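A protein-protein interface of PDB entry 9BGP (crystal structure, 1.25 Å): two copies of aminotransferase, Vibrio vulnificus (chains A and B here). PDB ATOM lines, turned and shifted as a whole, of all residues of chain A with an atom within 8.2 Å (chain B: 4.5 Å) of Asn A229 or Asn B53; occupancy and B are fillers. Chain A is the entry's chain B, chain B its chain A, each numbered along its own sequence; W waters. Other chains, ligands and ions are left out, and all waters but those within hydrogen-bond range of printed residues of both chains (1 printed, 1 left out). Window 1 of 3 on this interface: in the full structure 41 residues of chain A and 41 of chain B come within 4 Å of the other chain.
Glu B191 touches Val A27 (OE2 to CG1, 3.9 Å). His A212 touches Thr B55 (CE1 to OG1, 3.2 Å). Thr B55 touches Asn A229. N of Glu B191 touches CG2 of Thr A233 (3.4 Å).
Water W1 lies within hydrogen-bond range of OE2 of Glu B191 (2.6 Å), N of His A28 (2.8 Å) and O of Leu A232 (2.9 Å).
Positions printed for both chains: 51, 52, 53 and 56. Of the 8 pairs that touch across the chains among the printed residues, none has its exchanged pair printed and touching as well.
The side-chain amide nitrogen of Asn B53 lies within hydrogen-bond range of the backbone carbonyl oxygen of Asn A229 (2.9 Å). OP2 of LLP B185 lies within hydrogen-bond range of the side-chain amide nitrogen (ND2) of Asn A229, at 2.9 Å. The side-chain amide nitrogen (ND2) of Asn A229 sits at hydrogen-bond distance from the side-chain carboxylate (OE1) of Glu B191 (3.1 Å). OE2 of Glu B191 is in salt-bridge range of NE of Arg A231 (2.8 Å).
Printed residues of chain A that touch a printed residue of chain B: Val A27, His A212, Asn A229, Arg A231 and Thr A233. Among the printed residues, 8 pairs touch across the chains. Among the printed residues, Asp or Glu carboxylates within 4 Å of a Lys or Arg side-chain nitrogen of the other chain: Arg A231 with Glu B191 (2.8 Å).
Asn A229 touches just these residues of chain B: Asn B53, Thr B55, LLP B185 and Glu B191. Of chain A, only Asn A229 comes within 4 Å of Asn B53. Printed residues of chain B within 4 Å of Arg A231: Glu B191 (2.8 Å). Of the printed residues of chain A, LLP B185 touches Asn A229 (2.9 Å). Of the printed residues of chain A, Glu B191 touches Val A27 (3.9 Å), Asn A229 (3.1 Å), Arg A231 (2.8 Å) and Thr A233 (3.4 Å). Printed residues of chain A within 4 Å of Thr B55: His A212 and Asn A229. The nearest printed residue of chain B that does not touch Asn A229 is Gly B54 (5.3 Å).
The side-chain amide oxygen (OD1) of Asn B53 is in hydrogen-bond range of the backbone NH (N) of Thr B55, at 3.2 Å. The side-chain amide oxygen of Asn B53 lies within hydrogen-bond range of the backbone NH of Ala B56. N of Gly B54 lies within hydrogen-bond range of OP1 of LLP B185, at 2.8 Å. O of Arg A231 lies within hydrogen-bond range of OG of Ser A52. The side-chain hydroxyl (OG) of Ser A211 is in hydrogen-bond range of the guanidinium group (NH1) of Arg A231 (2.9 Å). N of Arg A231 lies within hydrogen-bond range of OD1 of Asn A229 (3.1 Å).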
ATOM      1  N   VAL A  27     -30.245 -20.401  29.229  1.00  0.00           N
ATOM      2  CA  VAL A  27     -30.831 -21.448  28.404  1.00  0.00           C
ATOM      3  C   VAL A  27     -32.347 -21.364  28.485  1.00  0.00           C
ATOM      4  O   VAL A  27     -32.894 -20.796  29.424  1.00  0.00           O
ATOM      5  CB  VAL A  27     -30.370 -22.878  28.748  1.00  0.00           C
ATOM      6  CG1 VAL A  27     -28.871 -23.059  28.536  1.00  0.00           C
ATOM      7  CG2 VAL A  27     -30.833 -23.327  30.130  1.00  0.00           C
ATOM      8  N   HIS A  28     -32.998 -21.978  27.494  1.00  0.00           N
ATOM      9  CA  HIS A  28     -34.449 -21.990  27.361  1.00  0.00           C
ATOM     10  C   HIS A  28     -35.085 -22.030  28.745  1.00  0.00           C
ATOM     11  O   HIS A  28     -34.924 -23.005  29.483  1.00  0.00           O
ATOM     12  CB  HIS A  28     -34.859 -23.221  26.558  1.00  0.00           C
ATOM     13  CG  HIS A  28     -36.325 -23.455  26.443  1.00  0.00           C
ATOM     14  ND1 HIS A  28     -36.925 -23.637  25.222  1.00  0.00           N
ATOM     15  CD2 HIS A  28     -37.292 -23.595  27.360  1.00  0.00           C
ATOM     16  CE1 HIS A  28     -38.224 -23.837  25.398  1.00  0.00           C
ATOM     17  NE2 HIS A  28     -38.485 -23.778  26.699  1.00  0.00           N
ATOM     18  N   VAL A  51     -37.389 -23.184  18.602  1.00  0.00           N
ATOM     19  CA  VAL A  51     -36.181 -23.878  18.204  1.00  0.00           C
ATOM     20  C   VAL A  51     -35.163 -22.895  17.614  1.00  0.00           C
ATOM     21  O   VAL A  51     -35.422 -21.708  17.431  1.00  0.00           O
ATOM     22  CB  VAL A  51     -36.497 -24.998  17.200  1.00  0.00           C
ATOM     23  CG1 VAL A  51     -37.359 -26.070  17.844  1.00  0.00           C
ATOM     24  CG2 VAL A  51     -37.163 -24.474  15.929  1.00  0.00           C
ATOM     25  N   SER A  52     -33.956 -23.392  17.306  1.00  0.00           N
ATOM     26  CA  SER A  52     -32.827 -22.565  16.909  1.00  0.00           C
ATOM     27  C   SER A  52     -33.086 -21.707  15.675  1.00  0.00           C
ATOM     28  O   SER A  52     -32.539 -20.605  15.593  1.00  0.00           O
ATOM     29  CB  SER A  52     -31.573 -23.386  16.665  1.00  0.00           C
ATOM     30  OG  SER A  52     -31.266 -24.212  17.768  1.00  0.00           O
ATOM     31  N   ASN A  53     -33.808 -22.239  14.675  1.00  0.00           N
ATOM     32  CA  ASN A  53     -34.074 -21.513  13.444  1.00  0.00           C
ATOM     33  C   ASN A  53     -35.179 -22.250  12.692  1.00  0.00           C
ATOM     34  O   ASN A  53     -35.633 -23.293  13.145  1.00  0.00           O
ATOM     35  CB  ASN A  53     -32.798 -21.309  12.632  1.00  0.00           C
ATOM     36  CG  ASN A  53     -32.057 -22.607  12.442  1.00  0.00           C
ATOM     37  OD1 ASN A  53     -32.559 -23.525  11.795  1.00  0.00           O
ATOM     38  ND2 ASN A  53     -30.854 -22.704  12.988  1.00  0.00           N
ATOM     39  N   ALA A  56     -34.245 -25.741  11.450  1.00  0.00           N
ATOM     40  CA  ALA A  56     -34.338 -26.693  12.529  1.00  0.00           C
ATOM     41  C   ALA A  56     -35.783 -27.146  12.708  1.00  0.00           C
ATOM     42  O   ALA A  56     -36.050 -28.305  13.004  1.00  0.00           O
ATOM     43  CB  ALA A  56     -33.887 -26.060  13.806  1.00  0.00           C
ATOM     44  N   LEU A  60     -36.828 -31.046  12.490  1.00  0.00           N
ATOM     45  CA  LEU A  60     -37.514 -31.758  13.560  1.00  0.00           C
ATOM     46  C   LEU A  60     -38.852 -32.343  13.114  1.00  0.00           C
ATOM     47  O   LEU A  60     -39.215 -33.449  13.532  1.00  0.00           O
ATOM     48  CB  LEU A  60     -37.702 -30.815  14.746  1.00  0.00           C
ATOM     49  CG  LEU A  60     -36.420 -30.472  15.493  1.00  0.00           C
ATOM     50  CD1 LEU A  60     -36.664 -29.229  16.345  1.00  0.00           C
ATOM     51  CD2 LEU A  60     -35.930 -31.646  16.330  1.00  0.00           C
ATOM     52  N   LEU A 208     -38.554 -34.017  22.647  1.00  0.00           N
ATOM     53  CA  LEU A 208     -37.414 -34.893  22.935  1.00  0.00           C
ATOM     54  C   LEU A 208     -36.274 -34.625  21.952  1.00  0.00           C
ATOM     55  O   LEU A 208     -35.116 -34.494  22.351  1.00  0.00           O
ATOM     56  CB  LEU A 208     -37.827 -36.355  22.798  1.00  0.00           C
ATOM     57  CG  LEU A 208     -38.801 -36.905  23.838  1.00  0.00           C
ATOM     58  CD1 LEU A 208     -39.279 -38.302  23.460  1.00  0.00           C
ATOM     59  CD2 LEU A 208     -38.195 -36.874  25.225  1.00  0.00           C
ATOM     60  N   LEU A 209     -36.598 -34.581  20.651  1.00  0.00           N
ATOM     61  CA  LEU A 209     -35.563 -34.439  19.646  1.00  0.00           C
ATOM     62  C   LEU A 209     -34.825 -33.115  19.751  1.00  0.00           C
ATOM     63  O   LEU A 209     -33.657 -33.027  19.366  1.00  0.00           O
ATOM     64  CB  LEU A 209     -36.171 -34.560  18.249  1.00  0.00           C
ATOM     65  CG  LEU A 209     -36.709 -35.937  17.890  1.00  0.00           C
ATOM     66  CD1 LEU A 209     -37.594 -35.856  16.649  1.00  0.00           C
ATOM     67  CD2 LEU A 209     -35.577 -36.920  17.670  1.00  0.00           C
ATOM     68  N   ARG A 210     -35.499 -32.087  20.273  1.00  0.00           N
ATOM     69  CA  ARG A 210     -34.928 -30.761  20.368  1.00  0.00           C
ATOM     70  C   ARG A 210     -33.796 -30.728  21.412  1.00  0.00           C
ATOM     71  O   ARG A 210     -32.970 -29.812  21.370  1.00  0.00           O
ATOM     72  CB  ARG A 210     -36.026 -29.736  20.721  1.00  0.00           C
ATOM     73  CG  ARG A 210     -35.573 -28.290  20.886  1.00  0.00           C
ATOM     74  CD  ARG A 210     -36.728 -27.390  21.269  1.00  0.00           C
ATOM     75  NE  ARG A 210     -37.227 -27.680  22.608  1.00  0.00           N
ATOM     76  CZ  ARG A 210     -38.239 -27.035  23.181  1.00  0.00           C
ATOM     77  NH1 ARG A 210     -38.801 -26.004  22.573  1.00  0.00           N
ATOM     78  NH2 ARG A 210     -38.709 -27.437  24.350  1.00  0.00           N
ATOM     79  N   SER A 211     -33.831 -31.654  22.390  1.00  0.00           N
ATOM     80  CA  SER A 211     -32.891 -31.591  23.503  1.00  0.00           C
ATOM     81  C   SER A 211     -32.420 -32.979  23.914  1.00  0.00           C
ATOM     82  O   SER A 211     -32.674 -33.411  25.035  1.00  0.00           O
ATOM     83  CB  SER A 211     -33.503 -30.849  24.686  1.00  0.00           C
ATOM     84  OG  SER A 211     -32.512 -30.595  25.682  1.00  0.00           O
ATOM     85  N   HIS A 212     -31.768 -33.675  22.985  1.00  0.00           N
ATOM     86  CA  HIS A 212     -30.927 -34.826  23.319  1.00  0.00           C
ATOM     87  C   HIS A 212     -31.749 -36.027  23.785  1.00  0.00           C
ATOM     88  O   HIS A 212     -31.203 -36.939  24.422  1.00  0.00           O
ATOM     89  CB  HIS A 212     -29.917 -34.474  24.416  1.00  0.00           C
ATOM     90  CG  HIS A 212     -29.111 -33.248  24.199  1.00  0.00           C
ATOM     91  ND1 HIS A 212     -28.173 -33.085  23.194  1.00  0.00           N
ATOM     92  CD2 HIS A 212     -29.110 -32.117  24.898  1.00  0.00           C
ATOM     93  CE1 HIS A 212     -27.635 -31.905  23.340  1.00  0.00           C
ATOM     94  NE2 HIS A 212     -28.205 -31.274  24.341  1.00  0.00           N
ATOM     95  N   GLY A 213     -33.050 -36.043  23.529  1.00  0.00           N
ATOM     96  CA  GLY A 213     -33.922 -37.101  23.990  1.00  0.00           C
ATOM     97  C   GLY A 213     -34.311 -36.993  25.454  1.00  0.00           C
ATOM     98  O   GLY A 213     -34.838 -37.946  26.018  1.00  0.00           O
ATOM     99  N   GLY A 227     -31.284 -37.742  20.036  1.00  0.00           N
ATOM    100  CA  GLY A 227     -31.764 -36.456  19.545  1.00  0.00           C
ATOM    101  C   GLY A 227     -30.618 -35.482  19.274  1.00  0.00           C
ATOM    102  O   GLY A 227     -29.449 -35.863  19.188  1.00  0.00           O
ATOM    103  N   LEU A 228     -31.005 -34.210  19.118  1.00  0.00           N
ATOM    104  CA  LEU A 228     -30.143 -33.096  18.723  1.00  0.00           C
ATOM    105  C   LEU A 228     -30.216 -32.015  19.790  1.00  0.00           C
ATOM    106  O   LEU A 228     -30.877 -32.150  20.808  1.00  0.00           O
ATOM    107  CB  LEU A 228     -30.657 -32.534  17.376  1.00  0.00           C
ATOM    108  CG  LEU A 228     -30.589 -33.507  16.204  1.00  0.00           C
ATOM    109  CD1 LEU A 228     -31.427 -33.010  15.015  1.00  0.00           C
ATOM    110  CD2 LEU A 228     -29.134 -33.714  15.785  1.00  0.00           C
ATOM    111  N   ASN A 229     -29.513 -30.907  19.533  1.00  0.00           N
ATOM    112  CA  ASN A 229     -29.707 -29.678  20.277  1.00  0.00           C
ATOM    113  C   ASN A 229     -30.176 -28.595  19.318  1.00  0.00           C
ATOM    114  O   ASN A 229     -29.405 -28.054  18.527  1.00  0.00           O
ATOM    115  CB  ASN A 229     -28.427 -29.205  20.954  1.00  0.00           C
ATOM    116  CG  ASN A 229     -28.639 -27.972  21.817  1.00  0.00           C
ATOM    117  OD1 ASN A 229     -29.696 -27.365  21.802  1.00  0.00           O
ATOM    118  ND2 ASN A 229     -27.626 -27.575  22.556  1.00  0.00           N
ATOM    119  N   TYR A 230     -31.462 -28.298  19.395  1.00  0.00           N
ATOM    120  CA  TYR A 230     -32.055 -27.193  18.656  1.00  0.00           C
ATOM    121  C   TYR A 230     -32.787 -26.250  19.605  1.00  0.00           C
ATOM    122  O   TYR A 230     -33.767 -25.602  19.238  1.00  0.00           O
ATOM    123  CB  TYR A 230     -32.949 -27.749  17.552  1.00  0.00           C
ATOM    124  CG  TYR A 230     -32.322 -28.142  16.228  1.00  0.00           C
ATOM    125  CD1 TYR A 230     -31.345 -27.369  15.635  1.00  0.00           C
ATOM    126  CD2 TYR A 230     -32.796 -29.209  15.485  1.00  0.00           C
ATOM    127  CE1 TYR A 230     -30.885 -27.656  14.365  1.00  0.00           C
ATOM    128  CE2 TYR A 230     -32.338 -29.524  14.224  1.00  0.00           C
ATOM    129  CZ  TYR A 230     -31.403 -28.703  13.634  1.00  0.00           C
ATOM    130  OH  TYR A 230     -30.962 -28.941  12.363  1.00  0.00           O
ATOM    131  N   ARG A 231     -32.274 -26.072  20.800  1.00  0.00           N
ATOM    132  CA  ARG A 231     -32.876 -25.169  21.754  1.00  0.00           C
ATOM    133  C   ARG A 231     -32.609 -23.704  21.431  1.00  0.00           C
ATOM    134  O   ARG A 231     -31.532 -23.351  20.969  1.00  0.00           O
ATOM    135  CB  ARG A 231     -32.327 -25.446  23.142  1.00  0.00           C
ATOM    136  CG  ARG A 231     -32.698 -26.837  23.636  1.00  0.00           C
ATOM    137  CD  ARG A 231     -32.291 -27.040  25.083  1.00  0.00           C
ATOM    138  NE  ARG A 231     -30.911 -26.682  25.292  1.00  0.00           N
ATOM    139  CZ  ARG A 231     -29.950 -27.514  25.655  1.00  0.00           C
ATOM    140  NH1 ARG A 231     -30.241 -28.788  25.898  1.00  0.00           N
ATOM    141  NH2 ARG A 231     -28.728 -27.040  25.831  1.00  0.00           N
ATOM    142  N   LEU A 232     -33.600 -22.859  21.696  1.00  0.00           N
ATOM    143  CA  LEU A 232     -33.470 -21.408  21.600  1.00  0.00           C
ATOM    144  C   LEU A 232     -33.099 -20.850  22.962  1.00  0.00           C
ATOM    145  O   LEU A 232     -33.592 -21.357  23.961  1.00  0.00           O
ATOM    146  CB  LEU A 232     -34.828 -20.856  21.148  1.00  0.00           C
ATOM    147  CG  LEU A 232     -34.826 -19.389  20.748  1.00  0.00           C
ATOM    148  CD1 LEU A 232     -33.933 -19.165  19.541  1.00  0.00           C
ATOM    149  CD2 LEU A 232     -36.223 -18.883  20.454  1.00  0.00           C
ATOM    150  N   THR A 233     -32.225 -19.841  23.022  1.00  0.00           N
ATOM    151  CA  THR A 233     -31.904 -19.252  24.316  1.00  0.00           C
ATOM    152  C   THR A 233     -33.104 -18.549  24.934  1.00  0.00           C
ATOM    153  O   THR A 233     -34.022 -18.115  24.235  1.00  0.00           O
ATOM    154  CB  THR A 233     -30.732 -18.270  24.252  1.00  0.00           C
ATOM    155  OG1 THR A 233     -31.095 -17.114  23.485  1.00  0.00           O
ATOM    156  CG2 THR A 233     -29.457 -18.881  23.712  1.00  0.00           C
ATOM    157  N   VAL B  51     -20.856 -21.827  15.807  1.00  0.00           N
ATOM    158  CA  VAL B  51     -22.070 -22.559  15.449  1.00  0.00           C
ATOM    159  C   VAL B  51     -23.067 -22.485  16.595  1.00  0.00           C
ATOM    160  O   VAL B  51     -22.781 -21.948  17.663  1.00  0.00           O
ATOM    161  CB  VAL B  51     -21.764 -24.016  15.045  1.00  0.00           C
ATOM    162  CG1 VAL B  51     -20.950 -24.102  13.760  1.00  0.00           C
ATOM    163  CG2 VAL B  51     -21.069 -24.760  16.181  1.00  0.00           C
ATOM    164  N   SER B  52     -24.271 -23.011  16.356  1.00  0.00           N
ATOM    165  CA  SER B  52     -25.397 -22.833  17.268  1.00  0.00           C
ATOM    166  C   SER B  52     -25.164 -23.409  18.672  1.00  0.00           C
ATOM    167  O   SER B  52     -25.676 -22.864  19.644  1.00  0.00           O
ATOM    168  CB  SER B  52     -26.673 -23.438  16.743  1.00  0.00           C
ATOM    169  OG  SER B  52     -26.970 -22.973  15.437  1.00  0.00           O
ATOM    170  N   ASN B  53     -24.421 -24.510  18.763  1.00  0.00           N
ATOM    171  CA  ASN B  53     -24.156 -25.162  20.041  1.00  0.00           C
ATOM    172  C   ASN B  53     -23.082 -26.225  19.798  1.00  0.00           C
ATOM    173  O   ASN B  53     -22.639 -26.436  18.668  1.00  0.00           O
ATOM    174  CB  ASN B  53     -25.440 -25.742  20.665  1.00  0.00           C
ATOM    175  CG  ASN B  53     -26.220 -26.606  19.698  1.00  0.00           C
ATOM    176  OD1 ASN B  53     -25.724 -27.635  19.252  1.00  0.00           O
ATOM    177  ND2 ASN B  53     -27.399 -26.176  19.289  1.00  0.00           N
ATOM    178  N   GLY B  54     -22.634 -26.867  20.887  1.00  0.00           N
ATOM    179  CA  GLY B  54     -21.552 -27.842  20.802  1.00  0.00           C
ATOM    180  C   GLY B  54     -21.977 -29.129  20.104  1.00  0.00           C
ATOM    181  O   GLY B  54     -21.153 -29.822  19.476  1.00  0.00           O
ATOM    182  N   THR B  55     -23.272 -29.481  20.219  1.00  0.00           N
ATOM    183  CA  THR B  55     -23.800 -30.653  19.524  1.00  0.00           C
ATOM    184  C   THR B  55     -23.742 -30.414  18.011  1.00  0.00           C
ATOM    185  O   THR B  55     -23.355 -31.289  17.227  1.00  0.00           O
ATOM    186  CB  THR B  55     -25.224 -30.979  19.983  1.00  0.00           C
ATOM    187  OG1 THR B  55     -25.213 -31.159  21.405  1.00  0.00           O
ATOM    188  CG2 THR B  55     -25.760 -32.214  19.307  1.00  0.00           C
ATOM    189  N   ALA B  56     -24.104 -29.200  17.588  1.00  0.00           N
ATOM    190  CA  ALA B  56     -24.017 -28.806  16.195  1.00  0.00           C
ATOM    191  C   ALA B  56     -22.575 -28.908  15.682  1.00  0.00           C
ATOM    192  O   ALA B  56     -22.318 -29.333  14.556  1.00  0.00           O
ATOM    193  CB  ALA B  56     -24.470 -27.360  16.072  1.00  0.00           C
ATOM    194  N   ALA B  57     -21.600 -28.550  16.520  1.00  0.00           N
ATOM    195  CA  ALA B  57     -20.193 -28.640  16.147  1.00  0.00           C
ATOM    196  C   ALA B  57     -19.824 -30.093  15.843  1.00  0.00           C
ATOM    197  O   ALA B  57     -19.240 -30.392  14.818  1.00  0.00           O
ATOM    198  CB  ALA B  57     -19.311 -28.064  17.236  1.00  0.00           C
ATOM    199  N1  LLP B 185     -20.422 -33.229  24.595  1.00  0.00           N
ATOM    200  C2  LLP B 185     -20.061 -33.105  25.866  1.00  0.00           C
ATOM    201  C2' LLP B 185     -18.960 -33.978  26.382  1.00  0.00           C
ATOM    202  C3  LLP B 185     -20.665 -32.153  26.680  1.00  0.00           C
ATOM    203  O3  LLP B 185     -20.272 -31.982  27.987  1.00  0.00           O
ATOM    204  C4  LLP B 185     -21.642 -31.292  26.139  1.00  0.00           C
ATOM    205  C4' LLP B 185     -22.147 -30.201  26.955  1.00  0.00           C
ATOM    206  C5  LLP B 185     -22.037 -31.478  24.803  1.00  0.00           C
ATOM    207  C6  LLP B 185     -21.403 -32.450  24.080  1.00  0.00           C
ATOM    208  C5' LLP B 185     -23.158 -30.697  24.173  1.00  0.00           C
ATOM    209  OP4 LLP B 185     -22.847 -29.300  23.926  1.00  0.00           O
ATOM    210  P   LLP B 185     -24.117 -28.310  23.807  1.00  0.00           P
ATOM    211  OP1 LLP B 185     -23.469 -26.978  23.505  1.00  0.00           O
ATOM    212  OP2 LLP B 185     -25.010 -28.804  22.718  1.00  0.00           O
ATOM    213  OP3 LLP B 185     -24.792 -28.302  25.169  1.00  0.00           O
ATOM    214  N   LLP B 185     -20.244 -24.195  30.774  1.00  0.00           N
ATOM    215  CA  LLP B 185     -18.946 -24.617  30.195  1.00  0.00           C
ATOM    216  CB  LLP B 185     -19.297 -25.319  28.881  1.00  0.00           C
ATOM    217  CG  LLP B 185     -20.161 -26.530  29.212  1.00  0.00           C
ATOM    218  CD  LLP B 185     -20.404 -27.583  28.149  1.00  0.00           C
ATOM    219  CE  LLP B 185     -21.615 -28.424  28.478  1.00  0.00           C
ATOM    220  NZ  LLP B 185     -21.468 -29.788  27.974  1.00  0.00           N
ATOM    221  C   LLP B 185     -17.994 -23.425  30.123  1.00  0.00           C
ATOM    222  O   LLP B 185     -17.085 -23.400  29.275  1.00  0.00           O
ATOM    223  N   GLU B 191     -26.374 -20.323  24.267  1.00  0.00           N
ATOM    224  CA  GLU B 191     -26.068 -21.530  23.530  1.00  0.00           C
ATOM    225  C   GLU B 191     -25.006 -21.122  22.523  1.00  0.00           C
ATOM    226  O   GLU B 191     -25.057 -20.020  21.989  1.00  0.00           O
ATOM    227  CB  GLU B 191     -27.295 -22.096  22.788  1.00  0.00           C
ATOM    228  CG  GLU B 191     -28.417 -22.573  23.691  1.00  0.00           C
ATOM    229  CD  GLU B 191     -28.358 -23.992  24.217  1.00  0.00           C
ATOM    230  OE1 GLU B 191     -27.393 -24.762  23.952  1.00  0.00           O
ATOM    231  OE2 GLU B 191     -29.368 -24.375  24.861  1.00  0.00           O
ATOM    232  N   GLY B 192     -24.083 -22.035  22.235  1.00  0.00           N
ATOM    233  CA  GLY B 192     -23.111 -21.745  21.193  1.00  0.00           C
ATOM    234  C   GLY B 192     -22.100 -22.869  21.121  1.00  0.00           C
ATOM    235  O   GLY B 192     -21.984 -23.664  22.043  1.00  0.00           O
ATOM    236  N   GLY B 193     -21.295 -22.852  20.073  1.00  0.00           N
ATOM    237  CA  GLY B 193     -20.168 -23.754  20.017  1.00  0.00           C
ATOM    238  C   GLY B 193     -19.217 -23.340  18.915  1.00  0.00           C
ATOM    239  O   GLY B 193     -19.425 -22.350  18.229  1.00  0.00           O
HETATM  240  O   HOH W   1     -31.408 -22.785  25.299  1.00  0.00           O
